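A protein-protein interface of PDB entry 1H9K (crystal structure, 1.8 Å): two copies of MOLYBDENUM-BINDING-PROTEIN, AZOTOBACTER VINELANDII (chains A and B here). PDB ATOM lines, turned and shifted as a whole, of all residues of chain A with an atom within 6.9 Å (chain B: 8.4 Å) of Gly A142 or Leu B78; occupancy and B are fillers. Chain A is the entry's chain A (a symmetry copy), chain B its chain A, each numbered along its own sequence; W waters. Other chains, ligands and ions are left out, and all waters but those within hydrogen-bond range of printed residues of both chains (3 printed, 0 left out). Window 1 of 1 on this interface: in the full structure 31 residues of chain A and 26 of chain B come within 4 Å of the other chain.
No position is printed for both chains.
Of the 19 pairs that touch across the chains among the printed residues, none has its exchanged pair printed and touching as well.
The side-chain amino group of Lys A13 lies within hydrogen-bond range of the side-chain hydroxyl of Tyr B76 (3.0 Å).
NH1 of Arg B77 lies within hydrogen-bond range of O of Ser A49.
The backbone NH (N) of Val A143 sits at hydrogen-bond distance from the backbone carbonyl oxygen (O) of Arg B77, 2.9 Å away.
The backbone carbonyl oxygen (O) of Ser B79 lies within hydrogen-bond range of the side-chain hydroxyl (OG) of Ser A46.
The backbone NH of Ser B79 sits at hydrogen-bond distance from the backbone carbonyl oxygen of Leu A141, at 2.7 Å.
The backbone carbonyl oxygen of Leu B68 lies within hydrogen-bond range of the backbone NH of Val B133 (2.8 Å).
The backbone carbonyl oxygen of Val A59 sits at hydrogen-bond distance from the backbone NH of Gly A142.
The backbone NH (N) of Val A61 sits at hydrogen-bond distance from the backbone carbonyl oxygen (O) of Ile A140, 2.6 Å away.
Of chain B, only Tyr B76 (3.9 Å), Arg B77 (3.2 Å) and Leu B78 (3.8 Å) come within 4 Å of Gly A142.
Of the printed residues of chain A, Leu B68 touches Val A61 (3.7 Å).
Printed residues of chain A within 4 Å of Tyr B76: Lys A13, Val A59, Gly A142, Val A143 and Pro A144.
Of chain A, only Leu A141 and Gly A142 come within 4 Å of Leu B78.
The nearest residue of chain B that does not touch Gly A142 is Ser B79 (4.9 Å).
The nearest residue of chain A that does not touch Leu B78 is Met A4 (4.04 Å).
Among the printed residues, merely in contact across the chains: Gly A142 with Arg B77, Val A143 with Tyr B76, Met A4 with Asp B72, Leu A141 with Leu B78, Val A59 with Tyr B76, Ile A6 with Leu B69, Pro A144 with Tyr B76, Pro A144 with Gly B75, Ile A140 with Ser B79, Val A61 with Leu B68, Leu A50 with Arg B77, Met A4 with Ser B73, Gly A142 with Leu B78 and Gly A142 with Tyr B76.
Of the 17 printed residues of chain A, 13 touch a printed residue of chain B.
Printed residues of chain A that touch a printed residue of chain B: Met A4, Ile A6, Lys A13, Ser A46, Ser A49, Leu A50, Val A59, Val A61, Ile A140, Leu A141, Gly A142, Val A143 and Pro A144.
Hydrophobic or aromatic side chains of chain A that line the printed part of chain B: Met A4, Ile A6, Leu A50, Val A59, Val A61, Ile A140, Leu A141, Val A143 and Pro A144.
Hydrophobic or aromatic side chains of chain B within 4 Å of the printed part of chain A: Leu B68, Tyr B76 and Leu B78.
Among the printed residues, no Asp or Glu carboxylate lies within 4 Å of a Lys or Arg side-chain nitrogen of the other chain.
Water W1 bridges O of Ser B79 (2.5 Å) and OG of Ser A46 (3.1 Å).
Water W2 lies within hydrogen-bond range of OG of Ser A46 and O of Ser B79.
Water W3 bridges the side-chain hydroxyl (OG) of Ser A46 (3.0 Å) and the backbone carbonyl oxygen (O) of Leu B78 (3.2 Å).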
ATOM      1  N   MET A   4       0.731 -11.636 -12.155  1.00  0.00           N
ATOM      2  CA  MET A   4      -0.626 -12.299 -12.177  1.00  0.00           C
ATOM      3  C   MET A   4      -1.122 -12.785 -10.821  1.00  0.00           C
ATOM      4  O   MET A   4      -0.257 -13.315 -10.097  1.00  0.00           O
ATOM      5  CB  MET A   4      -0.620 -13.436 -13.215  1.00  0.00           C
ATOM      6  CG  MET A   4      -1.671 -14.532 -12.922  1.00  0.00           C
ATOM      7  SD  MET A   4      -1.506 -15.875 -14.107  1.00  0.00           S
ATOM      8  CE  MET A   4      -2.760 -17.026 -13.628  1.00  0.00           C
ATOM      9  N   ILE A   6      -3.468 -15.047  -8.885  1.00  0.00           N
ATOM     10  CA  ILE A   6      -4.469 -16.112  -9.108  1.00  0.00           C
ATOM     11  C   ILE A   6      -4.423 -17.006  -7.870  1.00  0.00           C
ATOM     12  O   ILE A   6      -3.446 -17.113  -7.150  1.00  0.00           O
ATOM     13  CB  ILE A   6      -4.209 -16.850 -10.406  1.00  0.00           C
ATOM     14  CG1 ILE A   6      -5.299 -17.850 -10.799  1.00  0.00           C
ATOM     15  CG2 ILE A   6      -2.851 -17.565 -10.343  1.00  0.00           C
ATOM     16  CD1 ILE A   6      -5.454 -17.976 -12.334  1.00  0.00           C
ATOM     17  N   LYS A  13       6.835 -20.254 -13.733  1.00  0.00           N
ATOM     18  CA  LYS A  13       7.245 -19.694 -15.034  1.00  0.00           C
ATOM     19  C   LYS A  13       8.263 -20.642 -15.652  1.00  0.00           C
ATOM     20  O   LYS A  13       9.079 -21.303 -15.005  1.00  0.00           O
ATOM     21  CB  LYS A  13       7.755 -18.260 -14.898  1.00  0.00           C
ATOM     22  CG  LYS A  13       8.395 -17.607 -16.089  1.00  0.00           C
ATOM     23  CD  LYS A  13       7.559 -17.322 -17.325  1.00  0.00           C
ATOM     24  CE  LYS A  13       7.019 -15.911 -17.377  1.00  0.00           C
ATOM     25  NZ  LYS A  13       6.115 -15.663 -18.534  1.00  0.00           N
ATOM     26  N   SER A  46      -6.282 -23.246 -28.470  1.00  0.00           N
ATOM     27  CA  SER A  46      -5.475 -22.494 -27.530  1.00  0.00           C
ATOM     28  C   SER A  46      -4.014 -22.419 -27.949  1.00  0.00           C
ATOM     29  O   SER A  46      -3.382 -21.373 -27.779  1.00  0.00           O
ATOM     30  CB  SER A  46      -5.488 -23.122 -26.125  1.00  0.00           C
ATOM     31  OG  SER A  46      -6.772 -22.790 -25.590  1.00  0.00           O
ATOM     32  N   SER A  49      -4.039 -19.838 -30.667  1.00  0.00           N
ATOM     33  CA  SER A  49      -4.414 -18.485 -30.231  1.00  0.00           C
ATOM     34  C   SER A  49      -3.386 -17.940 -29.279  1.00  0.00           C
ATOM     35  O   SER A  49      -3.234 -16.701 -29.222  1.00  0.00           O
ATOM     36  CB  SER A  49      -5.831 -18.417 -29.644  1.00  0.00           C
ATOM     37  OG  SER A  49      -5.769 -18.548 -28.230  1.00  0.00           O
ATOM     38  N   LEU A  50      -2.784 -18.735 -28.392  1.00  0.00           N
ATOM     39  CA  LEU A  50      -1.745 -18.281 -27.484  1.00  0.00           C
ATOM     40  C   LEU A  50      -0.385 -18.113 -28.197  1.00  0.00           C
ATOM     41  O   LEU A  50       0.598 -17.689 -27.512  1.00  0.00           O
ATOM     42  CB  LEU A  50      -1.568 -19.232 -26.291  1.00  0.00           C
ATOM     43  CG  LEU A  50      -2.761 -19.442 -25.340  1.00  0.00           C
ATOM     44  CD1 LEU A  50      -2.459 -20.474 -24.272  1.00  0.00           C
ATOM     45  CD2 LEU A  50      -3.123 -18.125 -24.663  1.00  0.00           C
ATOM     46  N   LEU A  52       1.732 -20.406 -29.078  1.00  0.00           N
ATOM     47  CA  LEU A  52       2.740 -21.261 -28.517  1.00  0.00           C
ATOM     48  C   LEU A  52       3.773 -21.663 -29.578  1.00  0.00           C
ATOM     49  O   LEU A  52       3.490 -21.932 -30.737  1.00  0.00           O
ATOM     50  CB  LEU A  52       2.096 -22.502 -27.885  1.00  0.00           C
ATOM     51  CG  LEU A  52       1.081 -22.137 -26.768  1.00  0.00           C
ATOM     52  CD1 LEU A  52       0.561 -23.416 -26.141  1.00  0.00           C
ATOM     53  CD2 LEU A  52       1.692 -21.199 -25.738  1.00  0.00           C
ATOM     54  N   GLU A  57       8.306 -18.158 -23.469  1.00  0.00           N
ATOM     55  CA  GLU A  57       8.053 -18.207 -22.038  1.00  0.00           C
ATOM     56  C   GLU A  57       6.553 -18.341 -21.786  1.00  0.00           C
ATOM     57  O   GLU A  57       5.742 -17.762 -22.498  1.00  0.00           O
ATOM     58  CB  GLU A  57       8.538 -16.941 -21.302  1.00  0.00           C
ATOM     59  CG  GLU A  57      10.046 -17.032 -21.059  1.00  0.00           C
ATOM     60  CD  GLU A  57      10.561 -16.123 -19.963  1.00  0.00           C
ATOM     61  OE1 GLU A  57      10.388 -16.474 -18.771  1.00  0.00           O
ATOM     62  OE2 GLU A  57      11.151 -15.066 -20.290  1.00  0.00           O
ATOM     63  N   VAL A  58       6.231 -19.177 -20.802  1.00  0.00           N
ATOM     64  CA  VAL A  58       4.831 -19.406 -20.409  1.00  0.00           C
ATOM     65  C   VAL A  58       4.754 -19.475 -18.866  1.00  0.00           C
ATOM     66  O   VAL A  58       5.745 -19.644 -18.149  1.00  0.00           O
ATOM     67  CB  VAL A  58       4.278 -20.725 -20.947  1.00  0.00           C
ATOM     68  CG1 VAL A  58       4.081 -20.758 -22.464  1.00  0.00           C
ATOM     69  CG2 VAL A  58       5.203 -21.894 -20.558  1.00  0.00           C
ATOM     70  N   VAL A  59       3.535 -19.426 -18.330  1.00  0.00           N
ATOM     71  CA  VAL A  59       3.279 -19.738 -16.919  1.00  0.00           C
ATOM     72  C   VAL A  59       2.386 -20.979 -16.862  1.00  0.00           C
ATOM     73  O   VAL A  59       1.617 -21.177 -17.802  1.00  0.00           O
ATOM     74  CB  VAL A  59       2.638 -18.579 -16.131  1.00  0.00           C
ATOM     75  CG1 VAL A  59       3.526 -17.314 -16.189  1.00  0.00           C
ATOM     76  CG2 VAL A  59       1.259 -18.203 -16.609  1.00  0.00           C
ATOM     77  N   ALA A  60       2.642 -21.898 -15.940  1.00  0.00           N
ATOM     78  CA  ALA A  60       1.782 -23.110 -15.834  1.00  0.00           C
ATOM     79  C   ALA A  60       1.027 -22.930 -14.488  1.00  0.00           C
ATOM     80  O   ALA A  60       1.738 -22.647 -13.537  1.00  0.00           O
ATOM     81  CB  ALA A  60       2.631 -24.354 -15.839  1.00  0.00           C
ATOM     82  N   VAL A  61      -0.273 -23.168 -14.494  1.00  0.00           N
ATOM     83  CA  VAL A  61      -1.018 -22.951 -13.246  1.00  0.00           C
ATOM     84  C   VAL A  61      -1.675 -24.271 -12.849  1.00  0.00           C
ATOM     85  O   VAL A  61      -2.313 -24.898 -13.703  1.00  0.00           O
ATOM     86  CB  VAL A  61      -2.085 -21.857 -13.497  1.00  0.00           C
ATOM     87  CG1 VAL A  61      -2.977 -21.708 -12.273  1.00  0.00           C
ATOM     88  CG2 VAL A  61      -1.418 -20.504 -13.804  1.00  0.00           C
ATOM     89  N   ILE A 140      -3.173 -25.476 -16.496  1.00  0.00           N
ATOM     90  CA  ILE A 140      -3.607 -24.360 -17.309  1.00  0.00           C
ATOM     91  C   ILE A 140      -2.360 -23.573 -17.683  1.00  0.00           C
ATOM     92  O   ILE A 140      -1.479 -23.350 -16.842  1.00  0.00           O
ATOM     93  CB  ILE A 140      -4.602 -23.505 -16.489  1.00  0.00           C
ATOM     94  CG1 ILE A 140      -5.898 -24.364 -16.385  1.00  0.00           C
ATOM     95  CG2 ILE A 140      -4.960 -22.165 -17.119  1.00  0.00           C
ATOM     96  CD1 ILE A 140      -6.811 -23.799 -15.263  1.00  0.00           C
ATOM     97  N   LEU A 141      -2.321 -23.108 -18.919  1.00  0.00           N
ATOM     98  CA  LEU A 141      -1.183 -22.309 -19.358  1.00  0.00           C
ATOM     99  C   LEU A 141      -1.568 -20.855 -19.543  1.00  0.00           C
ATOM    100  O   LEU A 141      -2.715 -20.496 -19.821  1.00  0.00           O
ATOM    101  CB  LEU A 141      -0.675 -22.835 -20.722  1.00  0.00           C
ATOM    102  CG  LEU A 141       0.020 -24.184 -20.699  1.00  0.00           C
ATOM    103  CD1 LEU A 141       0.450 -24.554 -22.119  1.00  0.00           C
ATOM    104  CD2 LEU A 141       1.162 -24.169 -19.703  1.00  0.00           C
ATOM    105  N   GLY A 142      -0.554 -20.001 -19.310  1.00  0.00           N
ATOM    106  CA  GLY A 142      -0.792 -18.578 -19.531  1.00  0.00           C
ATOM    107  C   GLY A 142       0.375 -18.022 -20.384  1.00  0.00           C
ATOM    108  O   GLY A 142       1.505 -18.464 -20.164  1.00  0.00           O
ATOM    109  N   VAL A 143       0.104 -17.056 -21.214  1.00  0.00           N
ATOM    110  CA  VAL A 143       1.158 -16.418 -22.007  1.00  0.00           C
ATOM    111  C   VAL A 143       1.009 -14.910 -21.827  1.00  0.00           C
ATOM    112  O   VAL A 143      -0.008 -14.302 -21.702  1.00  0.00           O
ATOM    113  CB  VAL A 143       1.118 -16.796 -23.509  1.00  0.00           C
ATOM    114  CG1 VAL A 143       1.383 -18.289 -23.729  1.00  0.00           C
ATOM    115  CG2 VAL A 143      -0.171 -16.347 -24.182  1.00  0.00           C
ATOM    116  N   PRO A 144       2.298 -14.358 -21.662  1.00  0.00           N
ATOM    117  CA  PRO A 144       2.304 -12.896 -21.532  1.00  0.00           C
ATOM    118  C   PRO A 144       1.891 -12.326 -22.906  1.00  0.00           C
ATOM    119  O   PRO A 144       1.237 -11.256 -22.835  1.00  0.00           O
ATOM    120  CB  PRO A 144       3.708 -12.453 -21.209  1.00  0.00           C
ATOM    121  CG  PRO A 144       4.504 -13.683 -21.007  1.00  0.00           C
ATOM    122  CD  PRO A 144       3.781 -14.801 -21.675  1.00  0.00           C
ATOM    123  N   LEU B  68     -11.041 -21.547 -10.352  1.00  0.00           N
ATOM    124  CA  LEU B  68      -9.925 -20.738  -9.832  1.00  0.00           C
ATOM    125  C   LEU B  68     -10.401 -19.281  -9.787  1.00  0.00           C
ATOM    126  O   LEU B  68     -11.375 -18.932 -10.444  1.00  0.00           O
ATOM    127  CB  LEU B  68      -8.744 -20.740 -10.823  1.00  0.00           C
ATOM    128  CG  LEU B  68      -7.861 -21.987 -10.761  1.00  0.00           C
ATOM    129  CD1 LEU B  68      -8.571 -23.271 -11.139  1.00  0.00           C
ATOM    130  CD2 LEU B  68      -6.633 -21.826 -11.659  1.00  0.00           C
ATOM    131  N   LEU B  69      -9.796 -18.522  -8.884  1.00  0.00           N
ATOM    132  CA  LEU B  69     -10.175 -17.096  -8.822  1.00  0.00           C
ATOM    133  C   LEU B  69      -8.992 -16.267  -9.284  1.00  0.00           C
ATOM    134  O   LEU B  69      -7.872 -16.556  -8.833  1.00  0.00           O
ATOM    135  CB  LEU B  69     -10.592 -16.716  -7.412  1.00  0.00           C
ATOM    136  CG  LEU B  69     -11.927 -17.329  -6.952  1.00  0.00           C
ATOM    137  CD1 LEU B  69     -12.123 -16.937  -5.491  1.00  0.00           C
ATOM    138  CD2 LEU B  69     -13.052 -16.893  -7.874  1.00  0.00           C
ATOM    139  N   MET B  70      -9.210 -15.201 -10.051  1.00  0.00           N
ATOM    140  CA  MET B  70      -8.073 -14.390 -10.507  1.00  0.00           C
ATOM    141  C   MET B  70      -8.436 -12.922 -10.257  1.00  0.00           C
ATOM    142  O   MET B  70      -9.562 -12.542 -10.563  1.00  0.00           O
ATOM    143  CB  MET B  70      -7.833 -14.597 -12.007  1.00  0.00           C
ATOM    144  CG  MET B  70      -6.697 -13.757 -12.587  1.00  0.00           C
ATOM    145  SD  MET B  70      -6.191 -14.333 -14.203  1.00  0.00           S
ATOM    146  CE  MET B  70      -7.698 -14.254 -15.156  1.00  0.00           C
ATOM    147  N   ASP B  72      -5.905 -10.256 -10.973  1.00  0.00           N
ATOM    148  CA  ASP B  72      -5.088  -9.419 -11.857  1.00  0.00           C
ATOM    149  C   ASP B  72      -4.401 -10.374 -12.824  1.00  0.00           C
ATOM    150  O   ASP B  72      -3.631 -11.236 -12.403  1.00  0.00           O
ATOM    151  CB  ASP B  72      -4.112  -8.584 -11.058  1.00  0.00           C
ATOM    152  CG  ASP B  72      -3.403  -7.516 -11.869  1.00  0.00           C
ATOM    153  OD1 ASP B  72      -3.500  -7.489 -13.112  1.00  0.00           O
ATOM    154  OD2 ASP B  72      -2.750  -6.696 -11.206  1.00  0.00           O
ATOM    155  N   SER B  73      -4.838 -10.240 -14.080  1.00  0.00           N
ATOM    156  CA  SER B  73      -4.265 -11.105 -15.115  1.00  0.00           C
ATOM    157  C   SER B  73      -2.885 -10.613 -15.521  1.00  0.00           C
ATOM    158  O   SER B  73      -2.060 -11.336 -16.065  1.00  0.00           O
ATOM    159  CB  SER B  73      -5.229 -11.200 -16.305  1.00  0.00           C
ATOM    160  OG  SER B  73      -5.354  -9.932 -16.943  1.00  0.00           O
ATOM    161  N   GLY B  75      -2.033  -8.773 -17.935  1.00  0.00           N
ATOM    162  CA  GLY B  75      -1.770  -8.978 -19.352  1.00  0.00           C
ATOM    163  C   GLY B  75      -1.753 -10.413 -19.857  1.00  0.00           C
ATOM    164  O   GLY B  75      -1.814 -10.625 -21.084  1.00  0.00           O
ATOM    165  N   TYR B  76      -1.657 -11.390 -18.959  1.00  0.00           N
ATOM    166  CA  TYR B  76      -1.614 -12.790 -19.395  1.00  0.00           C
ATOM    167  C   TYR B  76      -2.926 -13.238 -20.021  1.00  0.00           C
ATOM    168  O   TYR B  76      -4.014 -12.875 -19.557  1.00  0.00           O
ATOM    169  CB  TYR B  76      -1.292 -13.685 -18.188  1.00  0.00           C
ATOM    170  CG  TYR B  76       0.199 -13.723 -17.906  1.00  0.00           C
ATOM    171  CD1 TYR B  76       0.793 -12.702 -17.165  1.00  0.00           C
ATOM    172  CD2 TYR B  76       0.999 -14.746 -18.361  1.00  0.00           C
ATOM    173  CE1 TYR B  76       2.150 -12.735 -16.938  1.00  0.00           C
ATOM    174  CE2 TYR B  76       2.370 -14.778 -18.158  1.00  0.00           C
ATOM    175  CZ  TYR B  76       2.935 -13.745 -17.415  1.00  0.00           C
ATOM    176  OH  TYR B  76       4.294 -13.791 -17.162  1.00  0.00           O
ATOM    177  N   ARG B  77      -2.810 -14.108 -21.020  1.00  0.00           N
ATOM    178  CA  ARG B  77      -3.946 -14.736 -21.674  1.00  0.00           C
ATOM    179  C   ARG B  77      -3.874 -16.203 -21.258  1.00  0.00           C
ATOM    180  O   ARG B  77      -2.740 -16.719 -21.233  1.00  0.00           O
ATOM    181  CB  ARG B  77      -3.869 -14.646 -23.203  1.00  0.00           C
ATOM    182  CG  ARG B  77      -3.994 -13.189 -23.678  1.00  0.00           C
ATOM    183  CD  ARG B  77      -3.826 -13.101 -25.197  1.00  0.00           C
ATOM    184  NE  ARG B  77      -2.457 -13.379 -25.638  1.00  0.00           N
ATOM    185  CZ  ARG B  77      -2.137 -13.981 -26.780  1.00  0.00           C
ATOM    186  NH1 ARG B  77      -3.088 -14.386 -27.619  1.00  0.00           N
ATOM    187  NH2 ARG B  77      -0.873 -14.217 -27.108  1.00  0.00           N
ATOM    188  N   LEU B  78      -4.988 -16.804 -20.872  1.00  0.00           N
ATOM    189  CA  LEU B  78      -4.885 -18.184 -20.357  1.00  0.00           C
ATOM    190  C   LEU B  78      -5.489 -19.203 -21.311  1.00  0.00           C
ATOM    191  O   LEU B  78      -6.291 -18.818 -22.167  1.00  0.00           O
ATOM    192  CB  LEU B  78      -5.647 -18.340 -19.029  1.00  0.00           C
ATOM    193  CG  LEU B  78      -5.305 -17.362 -17.913  1.00  0.00           C
ATOM    194  CD1 LEU B  78      -6.246 -17.521 -16.700  1.00  0.00           C
ATOM    195  CD2 LEU B  78      -3.848 -17.528 -17.483  1.00  0.00           C
ATOM    196  N   SER B  79      -5.128 -20.470 -21.134  1.00  0.00           N
ATOM    197  CA  SER B  79      -5.692 -21.510 -21.991  1.00  0.00           C
ATOM    198  C   SER B  79      -7.104 -21.903 -21.586  1.00  0.00           C
ATOM    199  O   SER B  79      -7.821 -22.492 -22.411  1.00  0.00           O
ATOM    200  CB  SER B  79      -4.829 -22.769 -21.958  1.00  0.00           C
ATOM    201  OG  SER B  79      -4.612 -23.289 -20.658  1.00  0.00           O
ATOM    202  N   ALA B  80      -7.481 -21.612 -20.331  1.00  0.00           N
ATOM    203  CA  ALA B  80      -8.874 -21.934 -19.957  1.00  0.00           C
ATOM    204  C   ALA B  80      -9.906 -21.105 -20.692  1.00  0.00           C
ATOM    205  O   ALA B  80      -9.749 -19.899 -20.842  1.00  0.00           O
ATOM    206  CB  ALA B  80      -9.043 -21.571 -18.446  1.00  0.00           C
ATOM    207  N   ARG B  81     -10.964 -21.744 -21.156  1.00  0.00           N
ATOM    208  CA  ARG B  81     -11.960 -21.032 -21.982  1.00  0.00           C
ATOM    209  C   ARG B  81     -12.833 -20.064 -21.224  1.00  0.00           C
ATOM    210  O   ARG B  81     -13.293 -19.086 -21.817  1.00  0.00           O
ATOM    211  CB  ARG B  81     -12.810 -22.166 -22.596  1.00  0.00           C
ATOM    212  N   ASN B  82     -13.142 -20.293 -19.957  1.00  0.00           N
ATOM    213  CA  ASN B  82     -14.073 -19.457 -19.206  1.00  0.00           C
ATOM    214  C   ASN B  82     -13.391 -18.544 -18.208  1.00  0.00           C
ATOM    215  O   ASN B  82     -12.739 -19.051 -17.305  1.00  0.00           O
ATOM    216  CB  ASN B  82     -15.034 -20.353 -18.400  1.00  0.00           C
ATOM    217  CG  ASN B  82     -15.806 -21.238 -19.340  1.00  0.00           C
ATOM    218  OD1 ASN B  82     -16.535 -20.715 -20.224  1.00  0.00           O
ATOM    219  ND2 ASN B  82     -15.637 -22.565 -19.250  1.00  0.00           N
ATOM    220  N   ILE B  83     -13.488 -17.232 -18.415  1.00  0.00           N
ATOM    221  CA  ILE B  83     -12.961 -16.220 -17.521  1.00  0.00           C
ATOM    222  C   ILE B  83     -14.126 -15.280 -17.184  1.00  0.00           C
ATOM    223  O   ILE B  83     -14.454 -14.462 -18.060  1.00  0.00           O
ATOM    224  CB  ILE B  83     -11.774 -15.450 -18.131  1.00  0.00           C
ATOM    225  CG1 ILE B  83     -10.613 -16.409 -18.386  1.00  0.00           C
ATOM    226  CG2 ILE B  83     -11.342 -14.412 -17.074  1.00  0.00           C
ATOM    227  CD1 ILE B  83      -9.421 -15.821 -19.087  1.00  0.00           C
ATOM    228  N   SER B 131     -12.231 -12.606 -11.174  1.00  0.00           N
ATOM    229  CA  SER B 131     -12.732 -13.443 -12.247  1.00  0.00           C
ATOM    230  C   SER B 131     -12.720 -14.902 -11.797  1.00  0.00           C
ATOM    231  O   SER B 131     -11.740 -15.340 -11.201  1.00  0.00           O
ATOM    232  CB  SER B 131     -11.821 -13.274 -13.464  1.00  0.00           C
ATOM    233  OG  SER B 131     -11.895 -11.923 -13.871  1.00  0.00           O
ATOM    234  N   ALA B 132     -13.700 -15.664 -12.199  1.00  0.00           N
ATOM    235  CA  ALA B 132     -13.703 -17.100 -11.947  1.00  0.00           C
ATOM    236  C   ALA B 132     -13.109 -17.674 -13.250  1.00  0.00           C
ATOM    237  O   ALA B 132     -13.634 -17.464 -14.339  1.00  0.00           O
ATOM    238  CB  ALA B 132     -15.115 -17.568 -11.743  1.00  0.00           C
ATOM    239  N   VAL B 133     -12.142 -18.568 -13.090  1.00  0.00           N
ATOM    240  CA  VAL B 133     -11.479 -19.156 -14.264  1.00  0.00           C
ATOM    241  C   VAL B 133     -11.876 -20.628 -14.225  1.00  0.00           C
ATOM    242  O   VAL B 133     -11.620 -21.263 -13.194  1.00  0.00           O
ATOM    243  CB  VAL B 133      -9.960 -18.975 -14.158  1.00  0.00           C
ATOM    244  CG1 VAL B 133      -9.279 -19.594 -15.397  1.00  0.00           C
ATOM    245  CG2 VAL B 133      -9.619 -17.476 -14.104  1.00  0.00           C
ATOM    246  N   ILE B 134     -12.533 -21.092 -15.297  1.00  0.00           N
ATOM    247  CA  ILE B 134     -12.985 -22.474 -15.340  1.00  0.00           C
ATOM    248  C   ILE B 134     -12.646 -23.140 -16.663  1.00  0.00           C
ATOM    249  O   ILE B 134     -12.946 -22.564 -17.686  1.00  0.00           O
ATOM    250  CB  ILE B 134     -14.511 -22.585 -15.149  1.00  0.00           C
ATOM    251  CG1 ILE B 134     -15.010 -21.843 -13.883  1.00  0.00           C
ATOM    252  CG2 ILE B 134     -14.903 -24.061 -15.044  1.00  0.00           C
ATOM    253  CD1 ILE B 134     -16.528 -21.727 -13.844  1.00  0.00           C
HETATM  254  O   HOH W   1      -9.528 -22.446 -24.300  1.00  0.00           O
HETATM  255  O   HOH W   2      -7.006 -25.190 -23.874  1.00  0.00           O
HETATM  256  O   HOH W   3      -6.898 -19.790 -25.143  1.00  0.00           O
